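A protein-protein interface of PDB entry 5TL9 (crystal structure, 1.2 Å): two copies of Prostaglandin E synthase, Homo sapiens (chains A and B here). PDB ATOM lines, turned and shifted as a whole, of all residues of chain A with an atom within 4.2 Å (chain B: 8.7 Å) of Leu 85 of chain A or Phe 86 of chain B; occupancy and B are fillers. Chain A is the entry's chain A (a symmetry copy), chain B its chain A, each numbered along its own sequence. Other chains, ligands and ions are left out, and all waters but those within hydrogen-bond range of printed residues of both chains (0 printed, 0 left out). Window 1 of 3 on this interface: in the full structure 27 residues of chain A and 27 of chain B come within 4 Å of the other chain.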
ATOM      1  N   PHE A  18      23.988 -23.987 -23.671  1.00  0.00           N
ATOM      2  CA  PHE A  18      23.154 -24.242 -22.507  1.00  0.00           C
ATOM      3  C   PHE A  18      22.264 -25.463 -22.723  1.00  0.00           C
ATOM      4  O   PHE A  18      22.182 -26.327 -21.853  1.00  0.00           O
ATOM      5  CB  PHE A  18      22.289 -23.036 -22.131  1.00  0.00           C
ATOM      6  CG  PHE A  18      21.214 -23.385 -21.138  1.00  0.00           C
ATOM      7  CD1 PHE A  18      21.543 -23.682 -19.811  1.00  0.00           C
ATOM      8  CD2 PHE A  18      19.882 -23.514 -21.546  1.00  0.00           C
ATOM      9  CE1 PHE A  18      20.559 -24.056 -18.905  1.00  0.00           C
ATOM     10  CE2 PHE A  18      18.894 -23.892 -20.643  1.00  0.00           C
ATOM     11  CZ  PHE A  18      19.233 -24.157 -19.320  1.00  0.00           C
ATOM     12  N   LEU A  19      21.593 -25.510 -23.873  1.00  0.00           N
ATOM     13  CA  LEU A  19      20.662 -26.593 -24.168  1.00  0.00           C
ATOM     14  C   LEU A  19      21.366 -27.939 -24.288  1.00  0.00           C
ATOM     15  O   LEU A  19      20.832 -28.953 -23.842  1.00  0.00           O
ATOM     16  CB  LEU A  19      19.823 -26.279 -25.411  1.00  0.00           C
ATOM     17  CG  LEU A  19      18.829 -25.117 -25.276  1.00  0.00           C
ATOM     18  CD1 LEU A  19      18.154 -24.858 -26.615  1.00  0.00           C
ATOM     19  CD2 LEU A  19      17.788 -25.351 -24.188  1.00  0.00           C
ATOM     20  N   SER A  22      22.516 -28.898 -20.558  1.00  0.00           N
ATOM     21  CA  SER A  22      21.316 -29.205 -19.783  1.00  0.00           C
ATOM     22  C   SER A  22      20.744 -30.561 -20.131  1.00  0.00           C
ATOM     23  O   SER A  22      20.470 -31.372 -19.246  1.00  0.00           O
ATOM     24  CB  SER A  22      20.250 -28.152 -20.031  1.00  0.00           C
ATOM     25  OG  SER A  22      20.623 -26.947 -19.423  1.00  0.00           O
ATOM     26  N   ILE A  81      20.823 -29.685 -10.198  1.00  0.00           N
ATOM     27  CA  ILE A  81      20.618 -29.634 -11.647  1.00  0.00           C
ATOM     28  C   ILE A  81      19.331 -28.876 -11.983  1.00  0.00           C
ATOM     29  O   ILE A  81      19.317 -28.082 -12.927  1.00  0.00           O
ATOM     30  CB  ILE A  81      20.688 -31.033 -12.297  1.00  0.00           C
ATOM     31  CG1 ILE A  81      22.108 -31.604 -12.126  1.00  0.00           C
ATOM     32  CG2 ILE A  81      20.282 -30.975 -13.768  1.00  0.00           C
ATOM     33  CD1 ILE A  81      22.275 -33.064 -12.497  1.00  0.00           C
ATOM     34  N   TYR A  82      18.260 -29.099 -11.221  1.00  0.00           N
ATOM     35  CA  TYR A  82      17.014 -28.376 -11.491  1.00  0.00           C
ATOM     36  C   TYR A  82      17.191 -26.846 -11.369  1.00  0.00           C
ATOM     37  O   TYR A  82      16.777 -26.130 -12.278  1.00  0.00           O
ATOM     38  CB  TYR A  82      15.839 -28.915 -10.669  1.00  0.00           C
ATOM     39  CG  TYR A  82      15.458 -30.369 -10.942  1.00  0.00           C
ATOM     40  CD1 TYR A  82      15.823 -31.030 -12.129  1.00  0.00           C
ATOM     41  CD2 TYR A  82      14.694 -31.078 -10.013  1.00  0.00           C
ATOM     42  CE1 TYR A  82      15.448 -32.351 -12.361  1.00  0.00           C
ATOM     43  CE2 TYR A  82      14.319 -32.393 -10.240  1.00  0.00           C
ATOM     44  CZ  TYR A  82      14.694 -33.022 -11.416  1.00  0.00           C
ATOM     45  OH  TYR A  82      14.336 -34.325 -11.652  1.00  0.00           O
ATOM     46  N   PRO A  83      17.851 -26.343 -10.293  1.00  0.00           N
ATOM     47  CA  PRO A  83      18.156 -24.900 -10.270  1.00  0.00           C
ATOM     48  C   PRO A  83      18.977 -24.423 -11.469  1.00  0.00           C
ATOM     49  O   PRO A  83      18.703 -23.349 -12.000  1.00  0.00           O
ATOM     50  CB  PRO A  83      18.951 -24.728  -8.974  1.00  0.00           C
ATOM     51  CG  PRO A  83      18.412 -25.790  -8.084  1.00  0.00           C
ATOM     52  CD  PRO A  83      18.082 -26.953  -8.968  1.00  0.00           C
ATOM     53  N   PHE A  84      19.960 -25.212 -11.896  1.00  0.00           N
ATOM     54  CA  PHE A  84      20.745 -24.882 -13.087  1.00  0.00           C
ATOM     55  C   PHE A  84      19.895 -24.754 -14.352  1.00  0.00           C
ATOM     56  O   PHE A  84      20.147 -23.876 -15.184  1.00  0.00           O
ATOM     57  CB  PHE A  84      21.837 -25.919 -13.313  1.00  0.00           C
ATOM     58  CG  PHE A  84      22.619 -25.724 -14.588  1.00  0.00           C
ATOM     59  CD1 PHE A  84      23.695 -24.830 -14.642  1.00  0.00           C
ATOM     60  CD2 PHE A  84      22.289 -26.445 -15.742  1.00  0.00           C
ATOM     61  CE1 PHE A  84      24.422 -24.661 -15.818  1.00  0.00           C
ATOM     62  CE2 PHE A  84      23.009 -26.272 -16.922  1.00  0.00           C
ATOM     63  CZ  PHE A  84      24.074 -25.377 -16.959  1.00  0.00           C
ATOM     64  N   LEU A  85      18.910 -25.637 -14.518  1.00  0.00           N
ATOM     65  CA  LEU A  85      18.015 -25.571 -15.680  1.00  0.00           C
ATOM     66  C   LEU A  85      17.308 -24.222 -15.760  1.00  0.00           C
ATOM     67  O   LEU A  85      17.148 -23.658 -16.846  1.00  0.00           O
ATOM     68  CB  LEU A  85      16.991 -26.709 -15.671  1.00  0.00           C
ATOM     69  CG  LEU A  85      17.512 -28.148 -15.764  1.00  0.00           C
ATOM     70  CD1 LEU A  85      16.348 -29.123 -15.702  1.00  0.00           C
ATOM     71  CD2 LEU A  85      18.331 -28.403 -17.014  1.00  0.00           C
ATOM     72  N   PHE A  86      16.905 -23.705 -14.602  1.00  0.00           N
ATOM     73  CA  PHE A  86      16.316 -22.386 -14.515  1.00  0.00           C
ATOM     74  C   PHE A  86      17.339 -21.266 -14.724  1.00  0.00           C
ATOM     75  O   PHE A  86      17.168 -20.419 -15.607  1.00  0.00           O
ATOM     76  CB  PHE A  86      15.578 -22.215 -13.182  1.00  0.00           C
ATOM     77  CG  PHE A  86      14.966 -20.863 -13.023  1.00  0.00           C
ATOM     78  CD1 PHE A  86      13.795 -20.531 -13.710  1.00  0.00           C
ATOM     79  CD2 PHE A  86      15.583 -19.898 -12.226  1.00  0.00           C
ATOM     80  CE1 PHE A  86      13.235 -19.269 -13.585  1.00  0.00           C
ATOM     81  CE2 PHE A  86      15.022 -18.631 -12.096  1.00  0.00           C
ATOM     82  CZ  PHE A  86      13.855 -18.319 -12.788  1.00  0.00           C
ATOM     83  N   LEU A  87      18.391 -21.262 -13.908  1.00  0.00           N
ATOM     84  CA  LEU A  87      19.380 -20.182 -13.919  1.00  0.00           C
ATOM     85  C   LEU A  87      20.090 -20.058 -15.257  1.00  0.00           C
ATOM     86  O   LEU A  87      20.248 -18.958 -15.776  1.00  0.00           O
ATOM     87  CB  LEU A  87      20.422 -20.379 -12.813  1.00  0.00           C
ATOM     88  CG  LEU A  87      19.975 -20.327 -11.348  1.00  0.00           C
ATOM     89  CD1 LEU A  87      21.118 -20.789 -10.461  1.00  0.00           C
ATOM     90  CD2 LEU A  87      19.481 -18.946 -10.927  1.00  0.00           C
ATOM     91  N   PHE A  89      19.087 -21.070 -18.223  1.00  0.00           N
ATOM     92  CA  PHE A  89      18.165 -20.629 -19.268  1.00  0.00           C
ATOM     93  C   PHE A  89      18.028 -19.110 -19.261  1.00  0.00           C
ATOM     94  O   PHE A  89      18.194 -18.464 -20.300  1.00  0.00           O
ATOM     95  CB  PHE A  89      16.797 -21.310 -19.131  1.00  0.00           C
ATOM     96  CG  PHE A  89      15.829 -20.944 -20.225  1.00  0.00           C
ATOM     97  CD1 PHE A  89      15.957 -21.491 -21.506  1.00  0.00           C
ATOM     98  CD2 PHE A  89      14.793 -20.036 -19.984  1.00  0.00           C
ATOM     99  CE1 PHE A  89      15.067 -21.150 -22.519  1.00  0.00           C
ATOM    100  CE2 PHE A  89      13.901 -19.690 -20.994  1.00  0.00           C
ATOM    101  CZ  PHE A  89      14.037 -20.249 -22.262  1.00  0.00           C
ATOM    102  N   PHE B  18       1.495 -28.341 -24.715  1.00  0.00           N
ATOM    103  CA  PHE B  18       2.524 -28.517 -23.703  1.00  0.00           C
ATOM    104  C   PHE B  18       2.118 -27.862 -22.385  1.00  0.00           C
ATOM    105  O   PHE B  18       2.239 -28.478 -21.328  1.00  0.00           O
ATOM    106  CB  PHE B  18       3.883 -27.971 -24.149  1.00  0.00           C
ATOM    107  CG  PHE B  18       4.864 -27.866 -23.013  1.00  0.00           C
ATOM    108  CD1 PHE B  18       5.408 -29.019 -22.437  1.00  0.00           C
ATOM    109  CD2 PHE B  18       5.170 -26.623 -22.450  1.00  0.00           C
ATOM    110  CE1 PHE B  18       6.274 -28.928 -21.354  1.00  0.00           C
ATOM    111  CE2 PHE B  18       6.033 -26.526 -21.363  1.00  0.00           C
ATOM    112  CZ  PHE B  18       6.588 -27.680 -20.819  1.00  0.00           C
ATOM    113  N   SER B  22       1.462 -29.892 -18.921  1.00  0.00           N
ATOM    114  CA  SER B  22       2.383 -29.546 -17.842  1.00  0.00           C
ATOM    115  C   SER B  22       1.657 -29.057 -16.607  1.00  0.00           C
ATOM    116  O   SER B  22       1.912 -29.534 -15.502  1.00  0.00           O
ATOM    117  CB  SER B  22       3.340 -28.460 -18.300  1.00  0.00           C
ATOM    118  OG  SER B  22       4.248 -28.989 -19.226  1.00  0.00           O
ATOM    119  N   THR B  80      10.814 -37.090 -12.554  1.00  0.00           N
ATOM    120  CA  THR B  80      10.352 -37.279 -13.936  1.00  0.00           C
ATOM    121  C   THR B  80       9.598 -36.086 -14.506  1.00  0.00           C
ATOM    122  O   THR B  80       9.842 -35.682 -15.643  1.00  0.00           O
ATOM    123  CB  THR B  80       9.453 -38.521 -14.067  1.00  0.00           C
ATOM    124  OG1 THR B  80       8.384 -38.425 -13.118  1.00  0.00           O
ATOM    125  CG2 THR B  80      10.246 -39.792 -13.845  1.00  0.00           C
ATOM    126  N   ILE B  81       8.673 -35.530 -13.726  1.00  0.00           N
ATOM    127  CA  ILE B  81       7.847 -34.420 -14.203  1.00  0.00           C
ATOM    128  C   ILE B  81       8.687 -33.149 -14.354  1.00  0.00           C
ATOM    129  O   ILE B  81       8.524 -32.421 -15.337  1.00  0.00           O
ATOM    130  CB  ILE B  81       6.584 -34.217 -13.337  1.00  0.00           C
ATOM    131  CG1 ILE B  81       5.678 -35.456 -13.459  1.00  0.00           C
ATOM    132  CG2 ILE B  81       5.845 -32.942 -13.737  1.00  0.00           C
ATOM    133  CD1 ILE B  81       4.518 -35.516 -12.485  1.00  0.00           C
ATOM    134  N   TYR B  82       9.584 -32.879 -13.406  1.00  0.00           N
ATOM    135  CA  TYR B  82      10.428 -31.686 -13.523  1.00  0.00           C
ATOM    136  C   TYR B  82      11.295 -31.711 -14.801  1.00  0.00           C
ATOM    137  O   TYR B  82      11.307 -30.718 -15.525  1.00  0.00           O
ATOM    138  CB  TYR B  82      11.235 -31.418 -12.249  1.00  0.00           C
ATOM    139  CG  TYR B  82      10.411 -31.133 -10.996  1.00  0.00           C
ATOM    140  CD1 TYR B  82       9.071 -30.707 -11.060  1.00  0.00           C
ATOM    141  CD2 TYR B  82      10.992 -31.262  -9.733  1.00  0.00           C
ATOM    142  CE1 TYR B  82       8.347 -30.437  -9.901  1.00  0.00           C
ATOM    143  CE2 TYR B  82      10.273 -30.994  -8.577  1.00  0.00           C
ATOM    144  CZ  TYR B  82       8.955 -30.579  -8.668  1.00  0.00           C
ATOM    145  OH  TYR B  82       8.229 -30.316  -7.532  1.00  0.00           O
ATOM    146  N   PRO B  83      11.971 -32.847 -15.117  1.00  0.00           N
ATOM    147  CA  PRO B  83      12.661 -32.912 -16.419  1.00  0.00           C
ATOM    148  C   PRO B  83      11.742 -32.677 -17.618  1.00  0.00           C
ATOM    149  O   PRO B  83      12.139 -31.993 -18.559  1.00  0.00           O
ATOM    150  CB  PRO B  83      13.227 -34.333 -16.447  1.00  0.00           C
ATOM    151  CG  PRO B  83      13.471 -34.647 -15.015  1.00  0.00           C
ATOM    152  CD  PRO B  83      12.384 -33.963 -14.243  1.00  0.00           C
ATOM    153  N   PHE B  84      10.531 -33.224 -17.582  1.00  0.00           N
ATOM    154  CA  PHE B  84       9.549 -32.987 -18.644  1.00  0.00           C
ATOM    155  C   PHE B  84       9.202 -31.508 -18.822  1.00  0.00           C
ATOM    156  O   PHE B  84       9.032 -31.042 -19.953  1.00  0.00           O
ATOM    157  CB  PHE B  84       8.275 -33.779 -18.382  1.00  0.00           C
ATOM    158  CG  PHE B  84       7.163 -33.499 -19.363  1.00  0.00           C
ATOM    159  CD1 PHE B  84       7.115 -34.154 -20.598  1.00  0.00           C
ATOM    160  CD2 PHE B  84       6.151 -32.584 -19.048  1.00  0.00           C
ATOM    161  CE1 PHE B  84       6.079 -33.904 -21.497  1.00  0.00           C
ATOM    162  CE2 PHE B  84       5.120 -32.324 -19.948  1.00  0.00           C
ATOM    163  CZ  PHE B  84       5.088 -32.983 -21.175  1.00  0.00           C
ATOM    164  N   LEU B  85       9.070 -30.773 -17.716  1.00  0.00           N
ATOM    165  CA  LEU B  85       8.778 -29.337 -17.786  1.00  0.00           C
ATOM    166  C   LEU B  85       9.840 -28.594 -18.588  1.00  0.00           C
ATOM    167  O   LEU B  85       9.524 -27.692 -19.370  1.00  0.00           O
ATOM    168  CB  LEU B  85       8.633 -28.720 -16.393  1.00  0.00           C
ATOM    169  CG  LEU B  85       7.495 -29.223 -15.496  1.00  0.00           C
ATOM    170  CD1 LEU B  85       7.547 -28.518 -14.152  1.00  0.00           C
ATOM    171  CD2 LEU B  85       6.125 -29.044 -16.120  1.00  0.00           C
ATOM    172  N   PHE B  86      11.096 -28.990 -18.400  1.00  0.00           N
ATOM    173  CA  PHE B  86      12.195 -28.447 -19.170  1.00  0.00           C
ATOM    174  C   PHE B  86      12.197 -28.934 -20.622  1.00  0.00           C
ATOM    175  O   PHE B  86      12.183 -28.123 -21.555  1.00  0.00           O
ATOM    176  CB  PHE B  86      13.533 -28.752 -18.486  1.00  0.00           C
ATOM    177  CG  PHE B  86      14.709 -28.235 -19.246  1.00  0.00           C
ATOM    178  CD1 PHE B  86      15.016 -26.872 -19.233  1.00  0.00           C
ATOM    179  CD2 PHE B  86      15.485 -29.099 -20.019  1.00  0.00           C
ATOM    180  CE1 PHE B  86      16.092 -26.382 -19.955  1.00  0.00           C
ATOM    181  CE2 PHE B  86      16.568 -28.612 -20.744  1.00  0.00           C
ATOM    182  CZ  PHE B  86      16.859 -27.250 -20.718  1.00  0.00           C
ATOM    183  N   LEU B  87      12.225 -30.251 -20.807  1.00  0.00           N
ATOM    184  CA  LEU B  87      12.352 -30.849 -22.139  1.00  0.00           C
ATOM    185  C   LEU B  87      11.193 -30.483 -23.052  1.00  0.00           C
ATOM    186  O   LEU B  87      11.402 -30.125 -24.207  1.00  0.00           O
ATOM    187  CB  LEU B  87      12.461 -32.375 -22.050  1.00  0.00           C
ATOM    188  CG  LEU B  87      13.676 -32.997 -21.353  1.00  0.00           C
ATOM    189  CD1 LEU B  87      13.439 -34.487 -21.175  1.00  0.00           C
ATOM    190  CD2 LEU B  87      14.983 -32.737 -22.095  1.00  0.00           C
ATOM    191  N   GLY B  88       9.975 -30.567 -22.523  1.00  0.00           N
ATOM    192  CA  GLY B  88       8.776 -30.273 -23.299  1.00  0.00           C
ATOM    193  C   GLY B  88       8.692 -28.819 -23.722  1.00  0.00           C
ATOM    194  O   GLY B  88       8.221 -28.521 -24.824  1.00  0.00           O
ATOM    195  N   PHE B  89       9.147 -27.913 -22.857  1.00  0.00           N
ATOM    196  CA  PHE B  89       9.159 -26.487 -23.176  1.00  0.00           C
ATOM    197  C   PHE B  89      10.099 -26.203 -24.344  1.00  0.00           C
ATOM    198  O   PHE B  89       9.702 -25.566 -25.324  1.00  0.00           O
ATOM    199  CB  PHE B  89       9.529 -25.642 -21.950  1.00  0.00           C
ATOM    200  CG  PHE B  89       9.489 -24.159 -22.205  1.00  0.00           C
ATOM    201  CD1 PHE B  89       8.267 -23.480 -22.287  1.00  0.00           C
ATOM    202  CD2 PHE B  89      10.672 -23.435 -22.381  1.00  0.00           C
ATOM    203  CE1 PHE B  89       8.228 -22.111 -22.529  1.00  0.00           C
ATOM    204  CE2 PHE B  89      10.638 -22.065 -22.625  1.00  0.00           C
ATOM    205  CZ  PHE B  89       9.416 -21.402 -22.696  1.00  0.00           C
ATOM    206  N   VAL B  90      11.329 -26.703 -24.247  1.00  0.00           N
ATOM    207  CA  VAL B  90      12.325 -26.515 -25.296  1.00  0.00           C
ATOM    208  C   VAL B  90      11.850 -27.165 -26.601  1.00  0.00           C
ATOM    209  O   VAL B  90      11.893 -26.537 -27.668  1.00  0.00           O
ATOM    210  CB  VAL B  90      13.711 -27.056 -24.858  1.00  0.00           C
ATOM    211  CG1 VAL B  90      14.732 -26.954 -25.988  1.00  0.00           C
ATOM    212  CG2 VAL B  90      14.209 -26.312 -23.623  1.00  0.00           C
ATOM    213  N   TYR B  91      11.366 -28.402 -26.497  1.00  0.00           N
ATOM    214  CA  TYR B  91      10.872 -29.178 -27.637  1.00  0.00           C
ATOM    215  C   TYR B  91       9.744 -28.467 -28.384  1.00  0.00           C
ATOM    216  O   TYR B  91       9.690 -28.521 -29.614  1.00  0.00           O
ATOM    217  CB  TYR B  91      10.445 -30.567 -27.158  1.00  0.00           C
ATOM    218  CG  TYR B  91       9.693 -31.421 -28.144  1.00  0.00           C
ATOM    219  CD1 TYR B  91      10.350 -32.061 -29.203  1.00  0.00           C
ATOM    220  CD2 TYR B  91       8.321 -31.628 -27.990  1.00  0.00           C
ATOM    221  CE1 TYR B  91       9.648 -32.866 -30.097  1.00  0.00           C
ATOM    222  CE2 TYR B  91       7.613 -32.433 -28.866  1.00  0.00           C
ATOM    223  CZ  TYR B  91       8.275 -33.049 -29.915  1.00  0.00           C
ATOM    224  OH  TYR B  91       7.547 -33.838 -30.771  1.00  0.00           O
ATOM    225  N   SER B  92       8.875 -27.778 -27.646  1.00  0.00           N
ATOM    226  CA  SER B  92       7.784 -26.998 -28.240  1.00  0.00           C
ATOM    227  C   SER B  92       8.274 -25.941 -29.235  1.00  0.00           C
ATOM    228  O   SER B  92       7.550 -25.590 -30.167  1.00  0.00           O
ATOM    229  CB  SER B  92       6.942 -26.332 -27.153  1.00  0.00           C
ATOM    230  OG  SER B  92       6.214 -27.294 -26.413  1.00  0.00           O
ATOM    231  N   PHE B  93       9.501 -25.457 -29.047  1.00  0.00           N
ATOM    232  CA  PHE B  93      10.082 -24.417 -29.907  1.00  0.00           C
ATOM    233  C   PHE B  93      10.991 -24.928 -31.030  1.00  0.00           C
ATOM    234  O   PHE B  93      11.584 -24.130 -31.767  1.00  0.00           O
ATOM    235  CB  PHE B  93      10.803 -23.369 -29.055  1.00  0.00           C
ATOM    236  CG  PHE B  93       9.880 -22.521 -28.232  1.00  0.00           C
ATOM    237  CD1 PHE B  93       9.214 -21.432 -28.802  1.00  0.00           C
ATOM    238  CD2 PHE B  93       9.663 -22.804 -26.887  1.00  0.00           C
ATOM    239  CE1 PHE B  93       8.357 -20.644 -28.047  1.00  0.00           C
ATOM    240  CE2 PHE B  93       8.804 -22.020 -26.126  1.00  0.00           C
ATOM    241  CZ  PHE B  93       8.150 -20.938 -26.705  1.00  0.00           C
ATOM    242  N   PHE B 105       3.262 -35.365 -25.504  1.00  0.00           N
ATOM    243  CA  PHE B 105       2.728 -34.770 -24.278  1.00  0.00           C
ATOM    244  C   PHE B 105       1.631 -35.624 -23.644  1.00  0.00           C
ATOM    245  O   PHE B 105       1.607 -35.780 -22.423  1.00  0.00           O
ATOM    246  CB  PHE B 105       2.208 -33.345 -24.520  1.00  0.00           C
ATOM    247  CG  PHE B 105       3.197 -32.418 -25.192  1.00  0.00           C
ATOM    248  CD1 PHE B 105       4.577 -32.508 -24.955  1.00  0.00           C
ATOM    249  CD2 PHE B 105       2.736 -31.414 -26.042  1.00  0.00           C
ATOM    250  CE1 PHE B 105       5.469 -31.639 -25.581  1.00  0.00           C
ATOM    251  CE2 PHE B 105       3.622 -30.541 -26.664  1.00  0.00           C
ATOM    252  CZ  PHE B 105       4.988 -30.652 -26.436  1.00  0.00           C
ATOM    253  N   MET B 142      12.260 -36.583 -26.816  1.00  0.00           N
ATOM    254  CA  MET B 142      12.472 -35.134 -26.812  1.00  0.00           C
ATOM    255  C   MET B 142      13.916 -34.772 -26.486  1.00  0.00           C
ATOM    256  O   MET B 142      14.483 -33.888 -27.122  1.00  0.00           O
ATOM    257  CB  MET B 142      11.519 -34.429 -25.849  1.00  0.00           C
ATOM    258  CG  MET B 142      10.063 -34.502 -26.271  1.00  0.00           C
ATOM    259  SD  MET B 142       8.953 -33.573 -25.201  1.00  0.00           S
ATOM    260  CE  MET B 142       9.129 -34.435 -23.641  1.00  0.00           C
ATOM    261  N   ALA B 143      14.504 -35.464 -25.507  1.00  0.00           N
ATOM    262  CA  ALA B 143      15.897 -35.230 -25.129  1.00  0.00           C
ATOM    263  C   ALA B 143      16.843 -35.404 -26.322  1.00  0.00           C
ATOM    264  O   ALA B 143      17.691 -34.545 -26.569  1.00  0.00           O
ATOM    265  CB  ALA B 143      16.314 -36.125 -23.970  1.00  0.00           C
ATOM    266  N   ILE B 146      16.391 -32.524 -28.863  1.00  0.00           N
ATOM    267  CA  ILE B 146      17.039 -31.317 -28.356  1.00  0.00           C
ATOM    268  C   ILE B 146      18.558 -31.412 -28.510  1.00  0.00           C
ATOM    269  O   ILE B 146      19.198 -30.438 -28.925  1.00  0.00           O
ATOM    270  CB  ILE B 146      16.639 -31.010 -26.893  1.00  0.00           C
ATOM    271  CG1 ILE B 146      15.132 -30.726 -26.800  1.00  0.00           C
ATOM    272  CG2 ILE B 146      17.422 -29.813 -26.364  1.00  0.00           C
ATOM    273  CD1 ILE B 146      14.548 -30.845 -25.407  1.00  0.00           C
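The backbone carbonyl oxygen (O) of Phe 18 of chain A sits close to the side-chain hydroxyl (OG) of Ser 22 of chain A.
Phe 86 of chain B touches Phe 18 of chain A.
Leu 19 of chain A touches Val 90 of chain B (CD2 to CG2, 3.7 Å).
Ser 22 of chain A touches Phe 86 of chain B (CB to CZ, 3.6 Å).
CD2 of Tyr 82 of chain B touches CE2 of Tyr 82 of chain A, at 3.6 Å.
Tyr 82 of chain A touches Pro 83 of chain B (OH to CD, 3.3 Å).
Phe 86 of chain B touches Leu 85 of chain A.
Phe 89 of chain B touches Phe 89 of chain A (CE2 to CZ, 3.9 Å).
Of the printed residues of chain B, Phe 18 of chain A touches Phe 86.
Leu 85 of chain A touches one residue of chain B.
Of the printed residues of chain A, Tyr 82 of chain B touches Tyr 82 (3.6 Å).
Of the printed residues of chain A, Phe 86 of chain B touches Phe 18, Ser 22 and Leu 85.
The nearest residue of chain B that does not touch Leu 85 of chain A is Tyr 82 of chain B (5.3 Å).
Of the 20 printed residues of chain B, 5 touch a printed residue of chain A.
Hydrophobic or aromatic side chains of chain B within 4 Å of the printed part of chain A: Tyr 82, Pro 83, Phe 86, Phe 89 and Val 90.
Along chain B the printed residues that touch a printed residue of chain A span positions 82 to 90.
Printed residues of chain A that touch a printed residue of chain B: Phe 18, Leu 19, Ser 22, Tyr 82, Leu 85 and Phe 89.
Hydrophobic or aromatic side chains of chain A that line the printed part of chain B: Phe 18, Leu 19, Tyr 82, Leu 85 and Phe 89.
Phe 18 of chain A touches Phe 86 of chain B, but with the chains exchanged Phe 86 of chain A does not touch Phe 18 of chain B (12.4 Å).
Ser 22 of chain A touches Phe 86 of chain B, but with the chains exchanged Phe 86 of chain A does not touch Ser 22 of chain B (13.9 Å).
Tyr 82 of chain A touches its own counterpart, Tyr 82 of chain B.
Leu 85 of chain A touches Phe 86 of chain B, but with the chains exchanged Phe 86 of chain A does not touch Leu 85 of chain B (9.5 Å).
Positions printed for both chains: 18, 22, 81, 82, 83, 84, 85, 86, 87 and 89.
Of the 7 pairs that touch across the chains among the printed residues, 2 have their exchanged pair printed and touching as well.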
